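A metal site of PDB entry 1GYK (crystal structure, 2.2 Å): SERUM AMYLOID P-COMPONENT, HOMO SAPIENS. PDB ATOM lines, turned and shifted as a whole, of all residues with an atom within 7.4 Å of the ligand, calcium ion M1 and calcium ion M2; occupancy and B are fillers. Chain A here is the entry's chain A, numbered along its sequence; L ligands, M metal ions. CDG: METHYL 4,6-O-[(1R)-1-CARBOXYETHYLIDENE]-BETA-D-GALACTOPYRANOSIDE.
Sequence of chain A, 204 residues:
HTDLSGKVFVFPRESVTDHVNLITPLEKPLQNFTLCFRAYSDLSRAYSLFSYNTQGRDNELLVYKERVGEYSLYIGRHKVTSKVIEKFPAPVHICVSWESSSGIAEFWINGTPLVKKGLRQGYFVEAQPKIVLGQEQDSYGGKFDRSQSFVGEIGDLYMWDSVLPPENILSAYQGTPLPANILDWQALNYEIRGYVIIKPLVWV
Three residues have an atom within 4 Å of calcium ion M2: Glu 136, Asp 138 and Gln 148.
The nearest printed residue that does not touch calcium ion M2 is Asp 145 (4.3 Å).
Calcium ion M2 is bound by OE1 of Gln 148 (2.2 Å).
Calcium ion M2 is bound by the side-chain carboxylate (OE1) of Glu 136 (2.3 Å).
Calcium ion M2 is bound by an oxygen (O8A) of the ligand (2.4 Å).
Calcium ion M2 is bound by the side-chain carboxylate (OD2) of Asp 138 (2.4 Å).
The side-chain carboxylate (OD1) of Asp 138 binds calcium ion M2, at 2.7 Å.
Merely in contact with the ligand: Tyr 74 and Leu 62.
Hydrophobic or aromatic side chains within 4 Å of the ligand: Leu 62 and Tyr 74.
Within 4 Å of the ligand: Asp 58, Asn 59, Leu 62, Tyr 74, Glu 136, Asp 138 and Gln 148.
Along chain A the residues within 4 Å of the ligand span positions 58 to 148.
The nearest printed residue that does not touch the ligand is Tyr 64 (4.05 Å).
NE2 of Gln 137 sits at hydrogen-bond distance from O of Ser 51, 3.0 Å away.
The backbone carbonyl oxygen of Gln 148 lies within hydrogen-bond range of the backbone NH of Ser 48, at 3.1 Å.
NZ of Lys 79 lies within hydrogen-bond range of OH of Tyr 74 (3.1 Å).
The side-chain carboxylate (OD1) of Asp 58 lies close to the side-chain amide nitrogen (ND2) of Asn 53.
N of Tyr 74 is in hydrogen-bond range of O of Leu 62, 2.8 Å away.
The side-chain amide nitrogen of Gln 148 sits at hydrogen-bond distance from the side-chain hydroxyl of Tyr 64, at 3.1 Å.
The backbone NH of Asp 138 lies within hydrogen-bond range of the backbone carbonyl oxygen of Lys 143 (3.2 Å).
ND2 of Asn 53 lies close to O of Gln 137 (3.3 Å).
Within 4 Å of calcium ion M1: Asp 58, Asn 59, Glu 136, Gln 137 and Asp 138.
The nearest printed residue that does not touch calcium ion M1 is Asn 53 (4.6 Å).
Calcium ion M1 is bound by OD1 of Asn 59 (2.2 Å), OD1 of Asp 58 (2.3 Å), O of Gln 137 (2.4 Å), OD1 of Asp 138 (2.5 Å), O8B of the ligand (2.5 Å), OE2 of Glu 136 (2.6 Å), OE1 of Glu 136 (2.6 Å) and OD2 of Asp 58 (2.9 Å).
Calcium ion M1 has eight donor atoms within binding distance.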
ATOM      1  N   SER A  48      31.167  24.467  10.210  1.00  0.00           N
ATOM      2  CA  SER A  48      30.888  24.073  11.579  1.00  0.00           C
ATOM      3  C   SER A  48      32.186  24.106  12.394  1.00  0.00           C
ATOM      4  O   SER A  48      33.274  23.773  11.881  1.00  0.00           O
ATOM      5  CB  SER A  48      30.247  22.707  11.572  1.00  0.00           C
ATOM      6  OG  SER A  48      30.024  22.131  12.829  1.00  0.00           O
ATOM      7  N   SER A  51      30.116  20.442  16.662  1.00  0.00           N
ATOM      8  CA  SER A  51      28.898  19.671  16.362  1.00  0.00           C
ATOM      9  C   SER A  51      28.673  18.647  17.472  1.00  0.00           C
ATOM     10  O   SER A  51      29.499  17.795  17.707  1.00  0.00           O
ATOM     11  CB  SER A  51      28.983  18.994  14.979  1.00  0.00           C
ATOM     12  OG  SER A  51      27.827  18.263  14.623  1.00  0.00           O
ATOM     13  N   TYR A  52      27.512  18.754  18.117  1.00  0.00           N
ATOM     14  CA  TYR A  52      27.050  17.896  19.218  1.00  0.00           C
ATOM     15  C   TYR A  52      25.612  17.575  18.780  1.00  0.00           C
ATOM     16  O   TYR A  52      24.766  18.470  18.585  1.00  0.00           O
ATOM     17  CB  TYR A  52      27.157  18.725  20.532  1.00  0.00           C
ATOM     18  CG  TYR A  52      26.700  18.239  21.914  1.00  0.00           C
ATOM     19  CD1 TYR A  52      25.341  17.816  22.204  1.00  0.00           C
ATOM     20  CD2 TYR A  52      27.605  18.389  23.040  1.00  0.00           C
ATOM     21  CE1 TYR A  52      24.889  17.560  23.564  1.00  0.00           C
ATOM     22  CE2 TYR A  52      27.156  18.142  24.423  1.00  0.00           C
ATOM     23  CZ  TYR A  52      25.799  17.735  24.657  1.00  0.00           C
ATOM     24  OH  TYR A  52      25.402  17.489  25.944  1.00  0.00           O
ATOM     25  N   ASN A  53      25.393  16.265  18.635  1.00  0.00           N
ATOM     26  CA  ASN A  53      24.115  15.632  18.270  1.00  0.00           C
ATOM     27  C   ASN A  53      23.837  14.480  19.225  1.00  0.00           C
ATOM     28  O   ASN A  53      24.761  13.774  19.641  1.00  0.00           O
ATOM     29  CB  ASN A  53      24.169  15.014  16.856  1.00  0.00           C
ATOM     30  CG  ASN A  53      23.958  16.016  15.723  1.00  0.00           C
ATOM     31  OD1 ASN A  53      24.131  17.232  15.874  1.00  0.00           O
ATOM     32  ND2 ASN A  53      23.525  15.499  14.568  1.00  0.00           N
ATOM     33  N   ASP A  58      19.371  16.161  15.982  1.00  0.00           N
ATOM     34  CA  ASP A  58      20.304  16.941  15.145  1.00  0.00           C
ATOM     35  C   ASP A  58      20.314  18.400  15.573  1.00  0.00           C
ATOM     36  O   ASP A  58      19.251  18.947  15.785  1.00  0.00           O
ATOM     37  CB  ASP A  58      19.921  16.824  13.628  1.00  0.00           C
ATOM     38  CG  ASP A  58      20.902  17.565  12.675  1.00  0.00           C
ATOM     39  OD1 ASP A  58      22.125  17.493  12.880  1.00  0.00           O
ATOM     40  OD2 ASP A  58      20.429  18.270  11.760  1.00  0.00           O
ATOM     41  N   ASN A  59      21.501  19.033  15.569  1.00  0.00           N
ATOM     42  CA  ASN A  59      21.774  20.475  15.933  1.00  0.00           C
ATOM     43  C   ASN A  59      21.371  20.819  17.362  1.00  0.00           C
ATOM     44  O   ASN A  59      20.766  21.881  17.645  1.00  0.00           O
ATOM     45  CB  ASN A  59      21.159  21.488  14.917  1.00  0.00           C
ATOM     46  CG  ASN A  59      21.553  21.226  13.476  1.00  0.00           C
ATOM     47  OD1 ASN A  59      22.439  20.394  13.160  1.00  0.00           O
ATOM     48  ND2 ASN A  59      20.918  21.975  12.577  1.00  0.00           N
ATOM     49  N   GLU A  60      21.683  19.855  18.250  1.00  0.00           N
ATOM     50  CA  GLU A  60      21.394  19.926  19.682  1.00  0.00           C
ATOM     51  C   GLU A  60      22.235  21.015  20.368  1.00  0.00           C
ATOM     52  O   GLU A  60      21.721  21.746  21.230  1.00  0.00           O
ATOM     53  CB  GLU A  60      21.569  18.517  20.314  1.00  0.00           C
ATOM     54  CG  GLU A  60      21.231  18.327  21.861  1.00  0.00           C
ATOM     55  CD  GLU A  60      19.767  18.557  22.280  1.00  0.00           C
ATOM     56  OE1 GLU A  60      18.901  18.932  21.514  1.00  0.00           O
ATOM     57  OE2 GLU A  60      19.459  18.323  23.438  1.00  0.00           O
ATOM     58  N   LEU A  62      25.273  23.308  18.393  1.00  0.00           N
ATOM     59  CA  LEU A  62      26.114  23.626  17.250  1.00  0.00           C
ATOM     60  C   LEU A  62      26.649  25.068  17.196  1.00  0.00           C
ATOM     61  O   LEU A  62      25.871  26.009  17.189  1.00  0.00           O
ATOM     62  CB  LEU A  62      25.434  23.218  15.915  1.00  0.00           C
ATOM     63  CG  LEU A  62      25.972  23.570  14.515  1.00  0.00           C
ATOM     64  CD1 LEU A  62      27.211  22.774  14.212  1.00  0.00           C
ATOM     65  CD2 LEU A  62      24.942  23.308  13.504  1.00  0.00           C
ATOM     66  N   TYR A  64      28.403  27.411  14.703  1.00  0.00           N
ATOM     67  CA  TYR A  64      28.465  27.559  13.261  1.00  0.00           C
ATOM     68  C   TYR A  64      28.893  28.945  12.829  1.00  0.00           C
ATOM     69  O   TYR A  64      28.393  29.920  13.373  1.00  0.00           O
ATOM     70  CB  TYR A  64      27.043  27.274  12.715  1.00  0.00           C
ATOM     71  CG  TYR A  64      26.928  26.891  11.255  1.00  0.00           C
ATOM     72  CD1 TYR A  64      27.372  25.596  10.797  1.00  0.00           C
ATOM     73  CD2 TYR A  64      26.364  27.807  10.295  1.00  0.00           C
ATOM     74  CE1 TYR A  64      27.263  25.199   9.386  1.00  0.00           C
ATOM     75  CE2 TYR A  64      26.226  27.413   8.882  1.00  0.00           C
ATOM     76  CZ  TYR A  64      26.682  26.118   8.454  1.00  0.00           C
ATOM     77  OH  TYR A  64      26.538  25.702   7.152  1.00  0.00           O
ATOM     78  N   GLU A  66      28.708  31.558   9.895  1.00  0.00           N
ATOM     79  CA  GLU A  66      27.924  31.865   8.683  1.00  0.00           C
ATOM     80  C   GLU A  66      28.740  32.417   7.518  1.00  0.00           C
ATOM     81  O   GLU A  66      28.591  31.994   6.365  1.00  0.00           O
ATOM     82  CB  GLU A  66      26.795  32.860   8.996  1.00  0.00           C
ATOM     83  CG  GLU A  66      25.776  32.446  10.087  1.00  0.00           C
ATOM     84  CD  GLU A  66      24.882  31.227   9.731  1.00  0.00           C
ATOM     85  OE1 GLU A  66      24.612  30.957   8.525  1.00  0.00           O
ATOM     86  OE2 GLU A  66      24.456  30.536  10.683  1.00  0.00           O
ATOM     87  N   TYR A  74      23.328  27.071  17.905  1.00  0.00           N
ATOM     88  CA  TYR A  74      22.141  26.261  17.831  1.00  0.00           C
ATOM     89  C   TYR A  74      21.971  25.517  19.135  1.00  0.00           C
ATOM     90  O   TYR A  74      22.933  24.993  19.661  1.00  0.00           O
ATOM     91  CB  TYR A  74      22.203  25.243  16.704  1.00  0.00           C
ATOM     92  CG  TYR A  74      22.114  25.745  15.297  1.00  0.00           C
ATOM     93  CD1 TYR A  74      23.219  26.447  14.675  1.00  0.00           C
ATOM     94  CD2 TYR A  74      20.949  25.452  14.494  1.00  0.00           C
ATOM     95  CE1 TYR A  74      23.169  26.834  13.270  1.00  0.00           C
ATOM     96  CE2 TYR A  74      20.879  25.835  13.080  1.00  0.00           C
ATOM     97  CZ  TYR A  74      21.991  26.524  12.493  1.00  0.00           C
ATOM     98  OH  TYR A  74      21.887  26.891  11.175  1.00  0.00           O
ATOM     99  N   ARG A  77      17.761  22.650  17.646  1.00  0.00           N
ATOM    100  CA  ARG A  77      17.226  23.049  16.283  1.00  0.00           C
ATOM    101  C   ARG A  77      17.049  24.555  16.091  1.00  0.00           C
ATOM    102  O   ARG A  77      17.005  25.037  14.962  1.00  0.00           O
ATOM    103  CB  ARG A  77      15.906  22.344  15.828  1.00  0.00           C
ATOM    104  CG  ARG A  77      16.007  20.867  15.504  1.00  0.00           C
ATOM    105  CD  ARG A  77      14.810  20.051  16.042  1.00  0.00           C
ATOM    106  NE  ARG A  77      14.600  20.085  17.503  1.00  0.00           N
ATOM    107  CZ  ARG A  77      14.917  19.103  18.375  1.00  0.00           C
ATOM    108  NH1 ARG A  77      15.489  17.962  17.994  1.00  0.00           N
ATOM    109  NH2 ARG A  77      14.669  19.280  19.672  1.00  0.00           N
ATOM    110  N   LYS A  79      18.215  28.463  16.320  1.00  0.00           N
ATOM    111  CA  LYS A  79      19.447  29.254  16.174  1.00  0.00           C
ATOM    112  C   LYS A  79      19.368  30.684  16.693  1.00  0.00           C
ATOM    113  O   LYS A  79      18.268  31.245  16.883  1.00  0.00           O
ATOM    114  CB  LYS A  79      20.018  29.184  14.739  1.00  0.00           C
ATOM    115  CG  LYS A  79      19.253  29.920  13.609  1.00  0.00           C
ATOM    116  CD  LYS A  79      19.820  29.650  12.206  1.00  0.00           C
ATOM    117  CE  LYS A  79      21.186  30.280  11.921  1.00  0.00           C
ATOM    118  NZ  LYS A  79      21.708  29.892  10.565  1.00  0.00           N
ATOM    119  N   GLU A 136      30.236  18.623  10.367  1.00  0.00           N
ATOM    120  CA  GLU A 136      28.857  18.907  10.842  1.00  0.00           C
ATOM    121  C   GLU A 136      28.096  17.578  10.724  1.00  0.00           C
ATOM    122  O   GLU A 136      27.980  17.012   9.620  1.00  0.00           O
ATOM    123  CB  GLU A 136      28.158  19.934   9.909  1.00  0.00           C
ATOM    124  CG  GLU A 136      27.045  20.828  10.517  1.00  0.00           C
ATOM    125  CD  GLU A 136      25.752  20.134  10.878  1.00  0.00           C
ATOM    126  OE1 GLU A 136      25.130  19.506   9.984  1.00  0.00           O
ATOM    127  OE2 GLU A 136      25.414  20.157  12.080  1.00  0.00           O
ATOM    128  N   GLN A 137      27.434  17.192  11.813  1.00  0.00           N
ATOM    129  CA  GLN A 137      26.654  15.955  11.848  1.00  0.00           C
ATOM    130  C   GLN A 137      25.183  16.193  11.511  1.00  0.00           C
ATOM    131  O   GLN A 137      24.655  17.215  11.930  1.00  0.00           O
ATOM    132  CB  GLN A 137      26.674  15.306  13.233  1.00  0.00           C
ATOM    133  CG  GLN A 137      27.995  14.964  13.861  1.00  0.00           C
ATOM    134  CD  GLN A 137      27.834  14.686  15.345  1.00  0.00           C
ATOM    135  OE1 GLN A 137      27.485  13.587  15.753  1.00  0.00           O
ATOM    136  NE2 GLN A 137      28.086  15.694  16.154  1.00  0.00           N
ATOM    137  N   ASP A 138      24.604  15.300  10.680  1.00  0.00           N
ATOM    138  CA  ASP A 138      23.159  15.317  10.340  1.00  0.00           C
ATOM    139  C   ASP A 138      22.467  14.022  10.817  1.00  0.00           C
ATOM    140  O   ASP A 138      21.340  13.695  10.405  1.00  0.00           O
ATOM    141  CB  ASP A 138      22.843  15.654   8.862  1.00  0.00           C
ATOM    142  CG  ASP A 138      22.972  17.150   8.517  1.00  0.00           C
ATOM    143  OD1 ASP A 138      22.778  18.057   9.357  1.00  0.00           O
ATOM    144  OD2 ASP A 138      23.235  17.408   7.331  1.00  0.00           O
ATOM    145  N   SER A 139      23.186  13.303  11.696  1.00  0.00           N
ATOM    146  CA  SER A 139      22.758  12.074  12.390  1.00  0.00           C
ATOM    147  C   SER A 139      23.644  11.917  13.648  1.00  0.00           C
ATOM    148  O   SER A 139      24.402  12.850  13.995  1.00  0.00           O
ATOM    149  CB  SER A 139      22.839  10.841  11.474  1.00  0.00           C
ATOM    150  OG  SER A 139      24.159  10.428  11.230  1.00  0.00           O
ATOM    151  N   GLY A 142      27.379  10.730  12.236  1.00  0.00           N
ATOM    152  CA  GLY A 142      27.635  10.745  10.798  1.00  0.00           C
ATOM    153  C   GLY A 142      26.827  11.742  10.026  1.00  0.00           C
ATOM    154  O   GLY A 142      26.403  12.762  10.580  1.00  0.00           O
ATOM    155  N   LYS A 143      26.539  11.372   8.763  1.00  0.00           N
ATOM    156  CA  LYS A 143      25.789  12.160   7.748  1.00  0.00           C
ATOM    157  C   LYS A 143      26.368  13.608   7.525  1.00  0.00           C
ATOM    158  O   LYS A 143      25.751  14.657   7.806  1.00  0.00           O
ATOM    159  CB  LYS A 143      24.269  12.136   8.011  1.00  0.00           C
ATOM    160  CG  LYS A 143      23.537  10.937   7.426  1.00  0.00           C
ATOM    161  CD  LYS A 143      22.012  11.031   7.633  1.00  0.00           C
ATOM    162  CE  LYS A 143      21.294  12.014   6.693  1.00  0.00           C
ATOM    163  NZ  LYS A 143      21.414  11.608   5.259  1.00  0.00           N
ATOM    164  N   PHE A 144      27.638  13.602   7.121  1.00  0.00           N
ATOM    165  CA  PHE A 144      28.413  14.806   6.896  1.00  0.00           C
ATOM    166  C   PHE A 144      28.183  15.448   5.531  1.00  0.00           C
ATOM    167  O   PHE A 144      27.679  14.788   4.605  1.00  0.00           O
ATOM    168  CB  PHE A 144      29.912  14.515   7.120  1.00  0.00           C
ATOM    169  CG  PHE A 144      30.250  13.829   8.450  1.00  0.00           C
ATOM    170  CD1 PHE A 144      29.649  14.221   9.701  1.00  0.00           C
ATOM    171  CD2 PHE A 144      31.270  12.837   8.466  1.00  0.00           C
ATOM    172  CE1 PHE A 144      30.096  13.656  10.982  1.00  0.00           C
ATOM    173  CE2 PHE A 144      31.745  12.250   9.724  1.00  0.00           C
ATOM    174  CZ  PHE A 144      31.145  12.660  10.999  1.00  0.00           C
ATOM    175  N   ASP A 145      28.598  16.712   5.448  1.00  0.00           N
ATOM    176  CA  ASP A 145      28.498  17.559   4.260  1.00  0.00           C
ATOM    177  C   ASP A 145      29.833  18.297   4.056  1.00  0.00           C
ATOM    178  O   ASP A 145      30.232  19.107   4.902  1.00  0.00           O
ATOM    179  CB  ASP A 145      27.300  18.539   4.473  1.00  0.00           C
ATOM    180  CG  ASP A 145      26.889  19.334   3.224  1.00  0.00           C
ATOM    181  OD1 ASP A 145      27.483  19.224   2.113  1.00  0.00           O
ATOM    182  OD2 ASP A 145      25.961  20.133   3.368  1.00  0.00           O
ATOM    183  N   SER A 147      30.503  20.883   2.159  1.00  0.00           N
ATOM    184  CA  SER A 147      30.251  22.334   2.126  1.00  0.00           C
ATOM    185  C   SER A 147      30.219  23.003   3.505  1.00  0.00           C
ATOM    186  O   SER A 147      30.288  24.241   3.624  1.00  0.00           O
ATOM    187  CB  SER A 147      28.953  22.626   1.351  1.00  0.00           C
ATOM    188  OG  SER A 147      27.788  22.211   2.054  1.00  0.00           O
ATOM    189  N   GLN A 148      30.036  22.163   4.526  1.00  0.00           N
ATOM    190  CA  GLN A 148      29.992  22.569   5.921  1.00  0.00           C
ATOM    191  C   GLN A 148      31.276  22.142   6.679  1.00  0.00           C
ATOM    192  O   GLN A 148      31.386  22.419   7.876  1.00  0.00           O
ATOM    193  CB  GLN A 148      28.764  21.979   6.599  1.00  0.00           C
ATOM    194  CG  GLN A 148      27.422  22.392   6.035  1.00  0.00           C
ATOM    195  CD  GLN A 148      26.289  21.897   6.887  1.00  0.00           C
ATOM    196  OE1 GLN A 148      26.209  20.690   7.221  1.00  0.00           O
ATOM    197  NE2 GLN A 148      25.359  22.798   7.223  1.00  0.00           N
HETATM  198  C1  CDG L   1      19.525  25.692   6.667  1.00  0.00           C
HETATM  199  C4  CDG L   1      20.838  23.062   7.101  1.00  0.00           C
HETATM  200  C5  CDG L   1      19.606  23.536   7.923  1.00  0.00           C
HETATM  201  C6  CDG L   1      19.755  22.971   9.362  1.00  0.00           C
HETATM  202  C7  CDG L   1      22.293  23.188   9.194  1.00  0.00           C
HETATM  203  C8  CDG L   1      22.626  21.632   9.219  1.00  0.00           C
HETATM  204  C9  CDG L   1      23.515  23.746   9.861  1.00  0.00           C
HETATM  205  O2  CDG L   1      20.495  25.767   4.411  1.00  0.00           O
HETATM  206  O3  CDG L   1      21.924  23.235   4.937  1.00  0.00           O
HETATM  207  O4  CDG L   1      22.085  23.513   7.757  1.00  0.00           O
HETATM  208  O6  CDG L   1      21.033  23.362   9.970  1.00  0.00           O
HETATM  209  O8A CDG L   1      23.093  21.094   8.184  1.00  0.00           O
HETATM  210  O8B CDG L   1      22.364  20.960  10.241  1.00  0.00           O
HETATM  211 CA    CA M   1      23.173  19.027  11.585  1.00  0.00          CA
HETATM  212 CA    CA M   2      24.610  19.329   7.788  1.00  0.00          CA
